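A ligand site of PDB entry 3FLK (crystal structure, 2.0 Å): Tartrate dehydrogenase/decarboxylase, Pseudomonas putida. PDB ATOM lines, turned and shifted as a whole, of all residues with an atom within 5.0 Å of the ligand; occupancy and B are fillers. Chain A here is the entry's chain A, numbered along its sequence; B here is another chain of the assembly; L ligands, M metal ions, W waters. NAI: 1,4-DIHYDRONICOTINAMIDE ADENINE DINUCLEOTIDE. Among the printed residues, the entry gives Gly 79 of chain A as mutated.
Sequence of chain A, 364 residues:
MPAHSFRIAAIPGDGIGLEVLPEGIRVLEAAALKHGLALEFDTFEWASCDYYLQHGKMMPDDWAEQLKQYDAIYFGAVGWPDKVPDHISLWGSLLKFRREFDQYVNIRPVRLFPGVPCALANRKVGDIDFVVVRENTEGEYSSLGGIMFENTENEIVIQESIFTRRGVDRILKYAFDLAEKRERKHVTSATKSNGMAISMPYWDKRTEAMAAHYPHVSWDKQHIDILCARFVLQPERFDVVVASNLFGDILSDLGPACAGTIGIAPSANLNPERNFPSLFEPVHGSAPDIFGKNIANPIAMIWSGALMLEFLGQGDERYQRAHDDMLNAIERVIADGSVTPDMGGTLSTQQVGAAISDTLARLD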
ATOM      1  N   ILE A  16     -15.070   3.607  15.007  1.00  0.00           N
ATOM      2  CA  ILE A  16     -14.764   2.861  13.771  1.00  0.00           C
ATOM      3  C   ILE A  16     -14.956   1.354  13.913  1.00  0.00           C
ATOM      4  O   ILE A  16     -14.938   0.630  12.904  1.00  0.00           O
ATOM      5  CB  ILE A  16     -13.346   3.189  13.198  1.00  0.00           C
ATOM      6  CG1 ILE A  16     -12.235   2.639  14.100  1.00  0.00           C
ATOM      7  CG2 ILE A  16     -13.209   4.695  12.949  1.00  0.00           C
ATOM      8  CD1 ILE A  16     -10.910   2.477  13.382  1.00  0.00           C
ATOM      9  N   VAL A  20     -15.659  -1.007  10.715  1.00  0.00           N
ATOM     10  CA  VAL A  20     -14.808  -2.107  10.259  1.00  0.00           C
ATOM     11  C   VAL A  20     -15.410  -3.507  10.461  1.00  0.00           C
ATOM     12  O   VAL A  20     -15.149  -4.397   9.657  1.00  0.00           O
ATOM     13  CB  VAL A  20     -13.350  -2.029  10.829  1.00  0.00           C
ATOM     14  CG1 VAL A  20     -12.679  -0.710  10.418  1.00  0.00           C
ATOM     15  CG2 VAL A  20     -13.324  -2.207  12.353  1.00  0.00           C
ATOM     16  N   PHE A  75     -14.688  -8.723  18.075  1.00  0.00           N
ATOM     17  CA  PHE A  75     -14.828  -7.439  18.756  1.00  0.00           C
ATOM     18  C   PHE A  75     -14.219  -6.284  17.949  1.00  0.00           C
ATOM     19  O   PHE A  75     -13.122  -6.413  17.417  1.00  0.00           O
ATOM     20  CB  PHE A  75     -14.201  -7.519  20.151  1.00  0.00           C
ATOM     21  CG  PHE A  75     -14.311  -6.249  20.967  1.00  0.00           C
ATOM     22  CD1 PHE A  75     -15.505  -5.918  21.601  1.00  0.00           C
ATOM     23  CD2 PHE A  75     -13.206  -5.413  21.116  1.00  0.00           C
ATOM     24  CE1 PHE A  75     -15.603  -4.747  22.348  1.00  0.00           C
ATOM     25  CE2 PHE A  75     -13.298  -4.239  21.871  1.00  0.00           C
ATOM     26  CZ  PHE A  75     -14.492  -3.908  22.490  1.00  0.00           C
ATOM     27  N   GLY A  76     -14.947  -5.170  17.891  1.00  0.00           N
ATOM     28  CA  GLY A  76     -14.483  -3.994  17.165  1.00  0.00           C
ATOM     29  C   GLY A  76     -13.527  -3.160  17.997  1.00  0.00           C
ATOM     30  O   GLY A  76     -12.315  -3.371  17.956  1.00  0.00           O
ATOM     31  N   ALA A  77     -14.073  -2.220  18.758  1.00  0.00           N
ATOM     32  CA  ALA A  77     -13.300  -1.342  19.621  1.00  0.00           C
ATOM     33  C   ALA A  77     -14.195  -0.638  20.625  1.00  0.00           C
ATOM     34  O   ALA A  77     -15.387  -0.481  20.384  1.00  0.00           O
ATOM     35  CB  ALA A  77     -12.533  -0.315  18.791  1.00  0.00           C
ATOM     36  N   VAL A  78     -13.613  -0.206  21.736  1.00  0.00           N
ATOM     37  CA  VAL A  78     -14.383   0.480  22.771  1.00  0.00           C
ATOM     38  C   VAL A  78     -13.723   1.780  23.230  1.00  0.00           C
ATOM     39  O   VAL A  78     -12.507   1.833  23.441  1.00  0.00           O
ATOM     40  CB  VAL A  78     -14.682  -0.458  23.979  1.00  0.00           C
ATOM     41  CG1 VAL A  78     -13.413  -0.800  24.768  1.00  0.00           C
ATOM     42  CG2 VAL A  78     -15.739   0.148  24.888  1.00  0.00           C
ATOM     43  N   GLY A  79     -14.530   2.816  23.362  1.00  0.00           N
ATOM     44  CA  GLY A  79     -14.047   4.094  23.866  1.00  0.00           C
ATOM     45  C   GLY A  79     -14.638   5.272  23.131  1.00  0.00           C
ATOM     46  O   GLY A  79     -14.688   5.291  21.906  1.00  0.00           O
ATOM     47  N   TRP A  80     -15.117   6.252  23.900  1.00  0.00           N
ATOM     48  CA  TRP A  80     -15.589   7.516  23.358  1.00  0.00           C
ATOM     49  C   TRP A  80     -15.386   8.572  24.432  1.00  0.00           C
ATOM     50  O   TRP A  80     -16.316   8.899  25.170  1.00  0.00           O
ATOM     51  CB  TRP A  80     -17.065   7.408  22.930  1.00  0.00           C
ATOM     52  CG  TRP A  80     -17.444   8.472  21.953  1.00  0.00           C
ATOM     53  CD1 TRP A  80     -18.123   9.634  22.220  1.00  0.00           C
ATOM     54  CD2 TRP A  80     -17.161   8.488  20.552  1.00  0.00           C
ATOM     55  NE1 TRP A  80     -18.276  10.363  21.062  1.00  0.00           N
ATOM     56  CE2 TRP A  80     -17.696   9.692  20.022  1.00  0.00           C
ATOM     57  CE3 TRP A  80     -16.498   7.603  19.679  1.00  0.00           C
ATOM     58  CZ2 TRP A  80     -17.592  10.022  18.677  1.00  0.00           C
ATOM     59  CZ3 TRP A  80     -16.399   7.941  18.333  1.00  0.00           C
ATOM     60  CH2 TRP A  80     -16.941   9.142  17.839  1.00  0.00           C
ATOM     61  N   PRO A  81     -14.147   9.101  24.531  1.00  0.00           N
ATOM     62  CA  PRO A  81     -13.754  10.003  25.625  1.00  0.00           C
ATOM     63  C   PRO A  81     -14.569  11.302  25.725  1.00  0.00           C
ATOM     64  O   PRO A  81     -14.610  11.910  26.799  1.00  0.00           O
ATOM     65  CB  PRO A  81     -12.281  10.301  25.343  1.00  0.00           C
ATOM     66  CG  PRO A  81     -12.082   9.975  23.909  1.00  0.00           C
ATOM     67  CD  PRO A  81     -13.027   8.859  23.604  1.00  0.00           C
ATOM     68  N   ASP A  86     -12.005   7.115  29.456  1.00  0.00           N
ATOM     69  CA  ASP A  86     -11.360   5.936  28.863  1.00  0.00           C
ATOM     70  C   ASP A  86     -11.144   4.786  29.851  1.00  0.00           C
ATOM     71  O   ASP A  86     -11.222   3.613  29.460  1.00  0.00           O
ATOM     72  CB  ASP A  86     -10.022   6.318  28.202  1.00  0.00           C
ATOM     73  CG  ASP A  86     -10.195   6.948  26.818  1.00  0.00           C
ATOM     74  OD1 ASP A  86     -11.300   6.858  26.229  1.00  0.00           O
ATOM     75  OD2 ASP A  86      -9.226   7.558  26.330  1.00  0.00           O
ATOM     76  N   LEU A  90     -13.008   1.064  29.083  1.00  0.00           N
ATOM     77  CA  LEU A  90     -12.152  -0.108  28.884  1.00  0.00           C
ATOM     78  C   LEU A  90     -12.307  -1.149  29.997  1.00  0.00           C
ATOM     79  O   LEU A  90     -12.469  -2.335  29.710  1.00  0.00           O
ATOM     80  CB  LEU A  90     -10.679   0.298  28.728  1.00  0.00           C
ATOM     81  CG  LEU A  90      -9.758  -0.765  28.097  1.00  0.00           C
ATOM     82  CD1 LEU A  90      -9.998  -0.876  26.608  1.00  0.00           C
ATOM     83  CD2 LEU A  90      -8.292  -0.456  28.374  1.00  0.00           C
ATOM     84  N   LEU A  94     -13.916  -4.457  27.688  1.00  0.00           N
ATOM     85  CA  LEU A  94     -12.882  -5.323  27.114  1.00  0.00           C
ATOM     86  C   LEU A  94     -11.974  -5.978  28.154  1.00  0.00           C
ATOM     87  O   LEU A  94     -11.647  -7.160  28.034  1.00  0.00           O
ATOM     88  CB  LEU A  94     -12.032  -4.553  26.084  1.00  0.00           C
ATOM     89  CG  LEU A  94     -10.832  -5.254  25.426  1.00  0.00           C
ATOM     90  CD1 LEU A  94     -11.221  -6.517  24.655  1.00  0.00           C
ATOM     91  CD2 LEU A  94     -10.103  -4.285  24.532  1.00  0.00           C
ATOM     92  N   ARG A  98     -11.165  -9.971  28.836  1.00  0.00           N
ATOM     93  CA  ARG A  98      -9.801 -10.509  28.895  1.00  0.00           C
ATOM     94  C   ARG A  98      -9.513 -11.247  30.198  1.00  0.00           C
ATOM     95  O   ARG A  98      -8.909 -12.319  30.183  1.00  0.00           O
ATOM     96  CB  ARG A  98      -8.776  -9.405  28.678  1.00  0.00           C
ATOM     97  CG  ARG A  98      -8.711  -8.868  27.259  1.00  0.00           C
ATOM     98  CD  ARG A  98      -7.753  -7.696  27.160  1.00  0.00           C
ATOM     99  NE  ARG A  98      -7.530  -7.261  25.787  1.00  0.00           N
ATOM    100  CZ  ARG A  98      -6.922  -6.129  25.440  1.00  0.00           C
ATOM    101  NH1 ARG A  98      -6.478  -5.294  26.374  1.00  0.00           N
ATOM    102  NH2 ARG A  98      -6.769  -5.827  24.153  1.00  0.00           N
ATOM    103  N   ILE A 262      -0.938   1.445  11.583  1.00  0.00           N
ATOM    104  CA  ILE A 262      -1.565   0.646  12.640  1.00  0.00           C
ATOM    105  C   ILE A 262      -2.863  -0.009  12.152  1.00  0.00           C
ATOM    106  O   ILE A 262      -3.448  -0.828  12.849  1.00  0.00           O
ATOM    107  CB  ILE A 262      -1.793   1.465  13.969  1.00  0.00           C
ATOM    108  CG1 ILE A 262      -3.075   2.307  13.936  1.00  0.00           C
ATOM    109  CG2 ILE A 262      -0.539   2.266  14.362  1.00  0.00           C
ATOM    110  CD1 ILE A 262      -3.099   3.466  12.953  1.00  0.00           C
ATOM    111  N   GLY A 263      -3.281   0.351  10.943  1.00  0.00           N
ATOM    112  CA  GLY A 263      -4.570  -0.068  10.395  1.00  0.00           C
ATOM    113  C   GLY A 263      -4.711  -1.536   9.986  1.00  0.00           C
ATOM    114  O   GLY A 263      -5.817  -1.980   9.690  1.00  0.00           O
ATOM    115  N   GLU A 281      -9.898  -9.201  17.757  1.00  0.00           N
ATOM    116  CA  GLU A 281     -10.093  -7.762  17.594  1.00  0.00           C
ATOM    117  C   GLU A 281      -8.875  -7.137  16.921  1.00  0.00           C
ATOM    118  O   GLU A 281      -7.779  -7.694  16.959  1.00  0.00           O
ATOM    119  CB  GLU A 281     -10.322  -7.094  18.960  1.00  0.00           C
ATOM    120  CG  GLU A 281      -9.104  -7.173  19.894  1.00  0.00           C
ATOM    121  CD  GLU A 281      -9.195  -6.277  21.111  1.00  0.00           C
ATOM    122  OE1 GLU A 281      -9.913  -5.249  21.090  1.00  0.00           O
ATOM    123  OE2 GLU A 281      -8.527  -6.610  22.114  1.00  0.00           O
ATOM    124  N   PRO A 282      -9.056  -5.958  16.279  1.00  0.00           N
ATOM    125  CA  PRO A 282      -7.886  -5.203  15.858  1.00  0.00           C
ATOM    126  C   PRO A 282      -7.084  -4.673  17.044  1.00  0.00           C
ATOM    127  O   PRO A 282      -7.620  -4.532  18.155  1.00  0.00           O
ATOM    128  CB  PRO A 282      -8.477  -4.051  15.053  1.00  0.00           C
ATOM    129  CG  PRO A 282      -9.892  -3.950  15.472  1.00  0.00           C
ATOM    130  CD  PRO A 282     -10.316  -5.309  15.882  1.00  0.00           C
ATOM    131  N   VAL A 283      -5.804  -4.384  16.815  1.00  0.00           N
ATOM    132  CA  VAL A 283      -4.991  -3.688  17.808  1.00  0.00           C
ATOM    133  C   VAL A 283      -5.539  -2.274  18.047  1.00  0.00           C
ATOM    134  O   VAL A 283      -5.593  -1.812  19.193  1.00  0.00           O
ATOM    135  CB  VAL A 283      -3.492  -3.623  17.388  1.00  0.00           C
ATOM    136  CG1 VAL A 283      -2.692  -2.739  18.336  1.00  0.00           C
ATOM    137  CG2 VAL A 283      -2.891  -5.035  17.355  1.00  0.00           C
ATOM    138  N   HIS A 284      -5.959  -1.609  16.975  1.00  0.00           N
ATOM    139  CA  HIS A 284      -6.411  -0.201  17.039  1.00  0.00           C
ATOM    140  C   HIS A 284      -7.659   0.022  17.900  1.00  0.00           C
ATOM    141  O   HIS A 284      -8.416  -0.898  18.177  1.00  0.00           O
ATOM    142  CB  HIS A 284      -6.610   0.378  15.634  1.00  0.00           C
ATOM    143  CG  HIS A 284      -7.764  -0.222  14.873  1.00  0.00           C
ATOM    144  ND1 HIS A 284      -9.074  -0.049  15.251  1.00  0.00           N
ATOM    145  CD2 HIS A 284      -7.789  -0.953  13.736  1.00  0.00           C
ATOM    146  CE1 HIS A 284      -9.862  -0.667  14.392  1.00  0.00           C
ATOM    147  NE2 HIS A 284      -9.113  -1.224  13.461  1.00  0.00           N
ATOM    148  N   GLY A 285      -7.872   1.268  18.311  1.00  0.00           N
ATOM    149  CA  GLY A 285      -9.037   1.643  19.108  1.00  0.00           C
ATOM    150  C   GLY A 285     -10.208   2.112  18.269  1.00  0.00           C
ATOM    151  O   GLY A 285     -10.343   1.746  17.103  1.00  0.00           O
ATOM    152  N   SER A 286     -11.055   2.940  18.891  1.00  0.00           N
ATOM    153  CA  SER A 286     -12.289   3.412  18.256  1.00  0.00           C
ATOM    154  C   SER A 286     -12.092   4.586  17.291  1.00  0.00           C
ATOM    155  O   SER A 286     -13.030   4.965  16.586  1.00  0.00           O
ATOM    156  CB  SER A 286     -13.323   3.768  19.331  1.00  0.00           C
ATOM    157  OG  SER A 286     -12.828   4.782  20.186  1.00  0.00           O
ATOM    158  N   ALA A 287     -10.888   5.150  17.261  1.00  0.00           N
ATOM    159  CA  ALA A 287     -10.513   6.257  16.365  1.00  0.00           C
ATOM    160  C   ALA A 287     -11.617   7.318  16.157  1.00  0.00           C
ATOM    161  O   ALA A 287     -12.123   7.477  15.040  1.00  0.00           O
ATOM    162  CB  ALA A 287     -10.026   5.709  15.018  1.00  0.00           C
ATOM    163  N   PRO A 288     -11.973   8.053  17.230  1.00  0.00           N
ATOM    164  CA  PRO A 288     -13.057   9.048  17.164  1.00  0.00           C
ATOM    165  C   PRO A 288     -12.829  10.158  16.137  1.00  0.00           C
ATOM    166  O   PRO A 288     -13.794  10.687  15.600  1.00  0.00           O
ATOM    167  CB  PRO A 288     -13.084   9.638  18.585  1.00  0.00           C
ATOM    168  CG  PRO A 288     -12.444   8.609  19.440  1.00  0.00           C
ATOM    169  CD  PRO A 288     -11.377   8.000  18.581  1.00  0.00           C
ATOM    170  N   ILE A 290     -11.636   9.986  13.146  1.00  0.00           N
ATOM    171  CA  ILE A 290     -11.949   9.579  11.758  1.00  0.00           C
ATOM    172  C   ILE A 290     -13.294   8.857  11.609  1.00  0.00           C
ATOM    173  O   ILE A 290     -13.706   8.526  10.500  1.00  0.00           O
ATOM    174  CB  ILE A 290     -10.823   8.741  11.079  1.00  0.00           C
ATOM    175  CG1 ILE A 290     -10.545   7.437  11.844  1.00  0.00           C
ATOM    176  CG2 ILE A 290      -9.548   9.576  10.892  1.00  0.00           C
ATOM    177  CD1 ILE A 290      -9.899   6.345  11.009  1.00  0.00           C
ATOM    178  N   ILE A 295     -13.185   5.978   6.179  1.00  0.00           N
ATOM    179  CA  ILE A 295     -11.828   5.839   5.631  1.00  0.00           C
ATOM    180  C   ILE A 295     -10.977   4.925   6.518  1.00  0.00           C
ATOM    181  O   ILE A 295      -9.813   4.678   6.215  1.00  0.00           O
ATOM    182  CB  ILE A 295     -11.119   7.198   5.447  1.00  0.00           C
ATOM    183  CG1 ILE A 295     -11.094   7.980   6.767  1.00  0.00           C
ATOM    184  CG2 ILE A 295     -11.759   7.999   4.291  1.00  0.00           C
ATOM    185  CD1 ILE A 295     -10.074   9.100   6.812  1.00  0.00           C
ATOM    186  N   ALA A 296     -11.574   4.435   7.600  1.00  0.00           N
ATOM    187  CA  ALA A 296     -10.918   3.475   8.489  1.00  0.00           C
ATOM    188  C   ALA A 296     -10.477   2.228   7.722  1.00  0.00           C
ATOM    189  O   ALA A 296     -11.251   1.667   6.948  1.00  0.00           O
ATOM    190  CB  ALA A 296     -11.838   3.097   9.640  1.00  0.00           C
ATOM    191  N   ASN A 297      -9.228   1.824   7.932  1.00  0.00           N
ATOM    192  CA  ASN A 297      -8.680   0.599   7.358  1.00  0.00           C
ATOM    193  C   ASN A 297      -9.342  -0.616   8.016  1.00  0.00           C
ATOM    194  O   ASN A 297      -9.257  -0.790   9.237  1.00  0.00           O
ATOM    195  CB  ASN A 297      -7.159   0.566   7.584  1.00  0.00           C
ATOM    196  CG  ASN A 297      -6.447  -0.442   6.693  1.00  0.00           C
ATOM    197  OD1 ASN A 297      -7.034  -1.407   6.225  1.00  0.00           O
ATOM    198  ND2 ASN A 297      -5.155  -0.215   6.472  1.00  0.00           N
ATOM    199  N   ASP A 342      -4.630   5.640   4.827  1.00  0.00           N
ATOM    200  CA  ASP A 342      -3.518   5.394   5.768  1.00  0.00           C
ATOM    201  C   ASP A 342      -2.412   4.546   5.139  1.00  0.00           C
ATOM    202  O   ASP A 342      -1.278   4.522   5.624  1.00  0.00           O
ATOM    203  CB  ASP A 342      -4.023   4.756   7.073  1.00  0.00           C
ATOM    204  CG  ASP A 342      -4.636   3.385   6.864  1.00  0.00           C
ATOM    205  OD1 ASP A 342      -4.042   2.388   7.321  1.00  0.00           O
ATOM    206  OD2 ASP A 342      -5.710   3.312   6.239  1.00  0.00           O
ATOM    207  N   ASN B 194      -6.414   4.633  29.946  1.00  0.00           N
ATOM    208  CA  ASN B 194      -7.351   3.514  29.832  1.00  0.00           C
ATOM    209  C   ASN B 194      -6.899   2.303  30.642  1.00  0.00           C
ATOM    210  O   ASN B 194      -7.652   1.819  31.487  1.00  0.00           O
ATOM    211  CB  ASN B 194      -7.704   3.163  28.378  1.00  0.00           C
ATOM    212  CG  ASN B 194      -6.489   3.093  27.452  1.00  0.00           C
ATOM    213  OD1 ASN B 194      -5.361   2.832  27.884  1.00  0.00           O
ATOM    214  ND2 ASN B 194      -6.726   3.303  26.171  1.00  0.00           N
ATOM    215  N   HIS B 223      -2.178   8.517  24.271  1.00  0.00           N
ATOM    216  CA  HIS B 223      -1.883   7.230  24.874  1.00  0.00           C
ATOM    217  C   HIS B 223      -0.511   6.776  24.394  1.00  0.00           C
ATOM    218  O   HIS B 223      -0.158   6.945  23.219  1.00  0.00           O
ATOM    219  CB  HIS B 223      -2.947   6.193  24.516  1.00  0.00           C
ATOM    220  CG  HIS B 223      -4.270   6.436  25.176  1.00  0.00           C
ATOM    221  ND1 HIS B 223      -4.404   6.612  26.536  1.00  0.00           N
ATOM    222  CD2 HIS B 223      -5.528   6.502  24.673  1.00  0.00           C
ATOM    223  CE1 HIS B 223      -5.678   6.782  26.830  1.00  0.00           C
ATOM    224  NE2 HIS B 223      -6.375   6.723  25.719  1.00  0.00           N
ATOM    225  N   ASP B 225       1.033   4.090  23.599  1.00  0.00           N
ATOM    226  CA  ASP B 225       1.190   3.176  22.461  1.00  0.00           C
ATOM    227  C   ASP B 225       1.135   3.912  21.121  1.00  0.00           C
ATOM    228  O   ASP B 225       2.042   3.778  20.301  1.00  0.00           O
ATOM    229  CB  ASP B 225       0.198   2.007  22.516  1.00  0.00           C
ATOM    230  CG  ASP B 225      -1.258   2.434  22.577  1.00  0.00           C
ATOM    231  OD1 ASP B 225      -1.560   3.612  22.846  1.00  0.00           O
ATOM    232  OD2 ASP B 225      -2.121   1.567  22.356  1.00  0.00           O
ATOM    233  N   ILE B 226       0.097   4.721  20.917  1.00  0.00           N
ATOM    234  CA  ILE B 226      -0.010   5.487  19.675  1.00  0.00           C
ATOM    235  C   ILE B 226       0.994   6.651  19.598  1.00  0.00           C
ATOM    236  O   ILE B 226       1.404   7.041  18.513  1.00  0.00           O
ATOM    237  CB  ILE B 226      -1.479   5.944  19.381  1.00  0.00           C
ATOM    238  CG1 ILE B 226      -1.609   6.435  17.936  1.00  0.00           C
ATOM    239  CG2 ILE B 226      -1.953   6.992  20.405  1.00  0.00           C
ATOM    240  CD1 ILE B 226      -1.463   5.331  16.892  1.00  0.00           C
ATOM    241  N   ARG B 230       3.445   7.493  16.510  1.00  0.00           N
ATOM    242  CA  ARG B 230       3.529   8.819  15.894  1.00  0.00           C
ATOM    243  C   ARG B 230       4.948   9.382  15.842  1.00  0.00           C
ATOM    244  O   ARG B 230       5.260  10.208  14.975  1.00  0.00           O
ATOM    245  CB  ARG B 230       2.578   9.807  16.575  1.00  0.00           C
ATOM    246  CG  ARG B 230       1.105   9.552  16.248  1.00  0.00           C
ATOM    247  CD  ARG B 230       0.234  10.731  16.638  1.00  0.00           C
ATOM    248  NE  ARG B 230      -1.154  10.558  16.184  1.00  0.00           N
ATOM    249  CZ  ARG B 230      -2.151  10.195  16.973  1.00  0.00           C
ATOM    250  NH1 ARG B 230      -1.944   9.979  18.267  1.00  0.00           N
ATOM    251  NH2 ARG B 230      -3.379  10.058  16.480  1.00  0.00           N
HETATM  252  PA  NAI L   1      -6.807   4.655  18.194  1.00  0.00           P
HETATM  253  O1A NAI L   1      -6.176   3.368  17.807  1.00  0.00           O
HETATM  254  O2A NAI L   1      -8.285   4.580  18.197  1.00  0.00           O
HETATM  255  O5B NAI L   1      -6.340   5.791  17.165  1.00  0.00           O
HETATM  256  C5B NAI L   1      -5.010   6.241  17.077  1.00  0.00           C
HETATM  257  C4B NAI L   1      -4.765   6.875  15.709  1.00  0.00           C
HETATM  258  O4B NAI L   1      -4.706   5.861  14.719  1.00  0.00           O
HETATM  259  C3B NAI L   1      -5.873   7.835  15.305  1.00  0.00           C
HETATM  260  O3B NAI L   1      -5.295   8.954  14.682  1.00  0.00           O
HETATM  261  C2B NAI L   1      -6.707   7.035  14.327  1.00  0.00           C
HETATM  262  O2B NAI L   1      -7.285   7.853  13.334  1.00  0.00           O
HETATM  263  C1B NAI L   1      -5.712   6.041  13.739  1.00  0.00           C
HETATM  264  N9A NAI L   1      -6.361   4.762  13.415  1.00  0.00           N
HETATM  265  C8A NAI L   1      -6.760   3.792  14.302  1.00  0.00           C
HETATM  266  N7A NAI L   1      -7.310   2.784  13.601  1.00  0.00           N
HETATM  267  C5A NAI L   1      -7.279   3.083  12.290  1.00  0.00           C
HETATM  268  C6A NAI L   1      -7.694   2.399  11.157  1.00  0.00           C
HETATM  269  N6A NAI L   1      -8.256   1.196  11.265  1.00  0.00           N
HETATM  270  N1A NAI L   1      -7.521   2.983   9.916  1.00  0.00           N
HETATM  271  C2A NAI L   1      -6.933   4.225   9.794  1.00  0.00           C
HETATM  272  N3A NAI L   1      -6.513   4.887  10.934  1.00  0.00           N
HETATM  273  C4A NAI L   1      -6.685   4.328  12.161  1.00  0.00           C
HETATM  274  O3  NAI L   1      -6.201   5.052  19.639  1.00  0.00           O
HETATM  275  PN  NAI L   1      -6.433   6.403  20.487  1.00  0.00           P
HETATM  276  O1N NAI L   1      -6.727   7.543  19.597  1.00  0.00           O
HETATM  277  O2N NAI L   1      -5.281   6.517  21.403  1.00  0.00           O
HETATM  278  O5D NAI L   1      -7.738   6.057  21.368  1.00  0.00           O
HETATM  279  C5D NAI L   1      -9.046   6.303  20.911  1.00  0.00           C
HETATM  280  C4D NAI L   1     -10.048   5.544  21.781  1.00  0.00           C
HETATM  281  O4D NAI L   1      -9.944   4.157  21.546  1.00  0.00           O
HETATM  282  C3D NAI L   1      -9.841   5.752  23.276  1.00  0.00           C
HETATM  283  O3D NAI L   1     -11.105   5.843  23.869  1.00  0.00           O
HETATM  284  C2D NAI L   1      -9.141   4.481  23.732  1.00  0.00           C
HETATM  285  O2D NAI L   1      -9.429   4.170  25.080  1.00  0.00           O
HETATM  286  C1D NAI L   1      -9.733   3.453  22.769  1.00  0.00           C
HETATM  287  N1N NAI L   1      -8.900   2.266  22.527  1.00  0.00           N
HETATM  288  C2N NAI L   1      -9.520   1.051  22.620  1.00  0.00           C
HETATM  289  C3N NAI L   1      -8.814  -0.130  22.381  1.00  0.00           C
HETATM  290  C7N NAI L   1      -9.572  -1.410  22.231  1.00  0.00           C
HETATM  291  O7N NAI L   1     -10.985  -1.400  22.249  1.00  0.00           O
HETATM  292  N7N NAI L   1      -8.900  -2.551  22.084  1.00  0.00           N
HETATM  293  C4N NAI L   1      -7.467  -0.048  22.036  1.00  0.00           C
HETATM  294  C5N NAI L   1      -6.845   1.192  21.929  1.00  0.00           C
HETATM  295  C6N NAI L   1      -7.581   2.354  22.173  1.00  0.00           C
HETATM  296 MG    MG M   1      -2.706  -0.379  22.197  1.00  0.00          MG
HETATM  297  O   HOH W   1      -4.395   8.792  22.414  1.00  0.00           O
HETATM  298  O   HOH W   2      -4.061  -0.108  20.635  1.00  0.00           O
HETATM  299  O   HOH W   3      -7.094  10.893  14.454  1.00  0.00           O
HETATM  300  O   HOH W   4      -5.574   7.318   9.992  1.00  0.00           O
HETATM  301  O   HOH W   5      -8.941   9.327  14.778  1.00  0.00           O
HETATM  302  O   HOH W   6      -6.031   9.402  11.554  1.00  0.00           O
HETATM  303  O   HOH W   7      -6.451  -3.592  21.353  1.00  0.00           O
HETATM  304  O   HOH W   8      -8.327   9.562  21.495  1.00  0.00           O
HETATM  305  O   HOH W   9     -11.549   2.898  25.953  1.00  0.00           O
HETATM  306  O   HOH W  10      -8.407   9.102  17.665  1.00  0.00           O
HETATM  307  O   HOH W  11      -5.238   9.450  18.610  1.00  0.00           O
HETATM  308  O   HOH W  12      -4.189   4.035  21.798  1.00  0.00           O
HETATM  309  O   HOH W  13      -3.814   2.523  19.477  1.00  0.00           O
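The side-chain carboxylate (OD1) of Asp 86 is in hydrogen-bond range of an oxygen (O3D) of the ligand (2.6 Å). N of Gly 285 lies within hydrogen-bond range of O1A of the ligand (2.7 Å). An oxygen (O2A) of the ligand sits at hydrogen-bond distance from the backbone NH of Ala 287, at 2.8 Å. O3B of the ligand is in hydrogen-bond range of NH2 of Arg 230 of chain B (2.9 Å). The backbone NH (N) of Asn 297 lies within hydrogen-bond range of a nitrogen (N1A) of the ligand, at 2.9 Å. The backbone carbonyl oxygen (O) of Asn 297 is in hydrogen-bond range of a nitrogen (N6A) of the ligand (3.0 Å). An oxygen (O7N) of the ligand sits at hydrogen-bond distance from the backbone NH of Val 78 (2.9 Å). An oxygen (O2D) of the ligand is in hydrogen-bond range of the side-chain amide nitrogen (ND2) of Asn 194 of chain B, at 3.0 Å. The side-chain carboxylate (OE1) of Glu 281 sits at hydrogen-bond distance from a nitrogen (N7N) of the ligand (3.0 Å). The backbone NH (N) of Ser 286 is in hydrogen-bond range of an oxygen (O4D) of the ligand (3.1 Å). An oxygen (O4D) of the ligand is in hydrogen-bond range of the side-chain hydroxyl of Ser 286, at 3.2 Å. N6A of the ligand lies close to NE2 of His 284, at 3.4 Å.
The side-chain carboxylate of Asp 86 lies within hydrogen-bond range of a ring nitrogen (NE2) of His 223 of chain B (3.0 Å). OD1 of Asp 342 lies within hydrogen-bond range of ND2 of Asn 297 (3.0 Å). ND2 of Asn 194 of chain B sits at hydrogen-bond distance from NE2 of His 223 of chain B (3.5 Å). NH2 of Arg 98 lies within salt-bridge range of OE2 of Glu 281 (2.8 Å). OG of Ser 286 is in hydrogen-bond range of O of Gly 79 (2.6 Å). N of Ile 16 sits at hydrogen-bond distance from O of Ser 286 (2.9 Å).
Merely in contact with the ligand: Ile 16 (3.6 Å), Phe 75 (3.7 Å), Ala 77 (3.5 Å), Gly 79 (3.4 Å), Pro 81 (3.6 Å), Leu 94 (3.2 Å), Ile 262 (3.4 Å), Gly 263 (3.99 Å), Val 283 (3.8 Å), Pro 288 (3.7 Å), Ile 290 (3.6 Å), Ala 296 (3.7 Å), Asp 342 (3.8 Å), His 223 of chain B (3.3 Å) and Ile 226 of chain B (3.5 Å). Hydrophobic or aromatic side chains that line the ligand: Ile 16, Phe 75, Ala 77, Val 78, Pro 81, Leu 94, Ile 262, His 284, Ala 287, Pro 288, Ile 290, His 223 of chain B and Ile 226 of chain B. Within 4 Å of the ligand: Ile 16, Phe 75, Ala 77, Val 78, Gly 79, Pro 81, Asp 86, Leu 94, Ile 262, Gly 263, Glu 281, Val 283, His 284, Gly 285, Ser 286, Ala 287, Pro 288, Ile 290, Ala 296, Asn 297, Asp 342, Asn 194 of chain B, His 223 of chain B, Ile 226 of chain B and Arg 230 of chain B. The nearest printed residue that does not touch the ligand is Trp 80 (4.03 Å).
Water W11 bridges O1N of the ligand and NH2 of Arg 230 of chain B. Water W9 lies within hydrogen-bond range of O2D of the ligand and O of Val 78. Water W1 bridges an oxygen (O2N) of the ligand and the backbone NH of His 223 of chain B. Water W5 bridges an oxygen (O2B) of the ligand (2.6 Å) and the backbone NH of Ile 290 (3.2 Å). Water W12 lies within hydrogen-bond range of an oxygen (O2N) of the ligand (2.7 Å) and the side-chain carboxylate (OD1) of Asp 225 of chain B (2.9 Å). Water W7 lies within hydrogen-bond range of a nitrogen (N7N) of the ligand (2.8 Å) and the backbone carbonyl oxygen (O) of Val 283 (2.9 Å).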
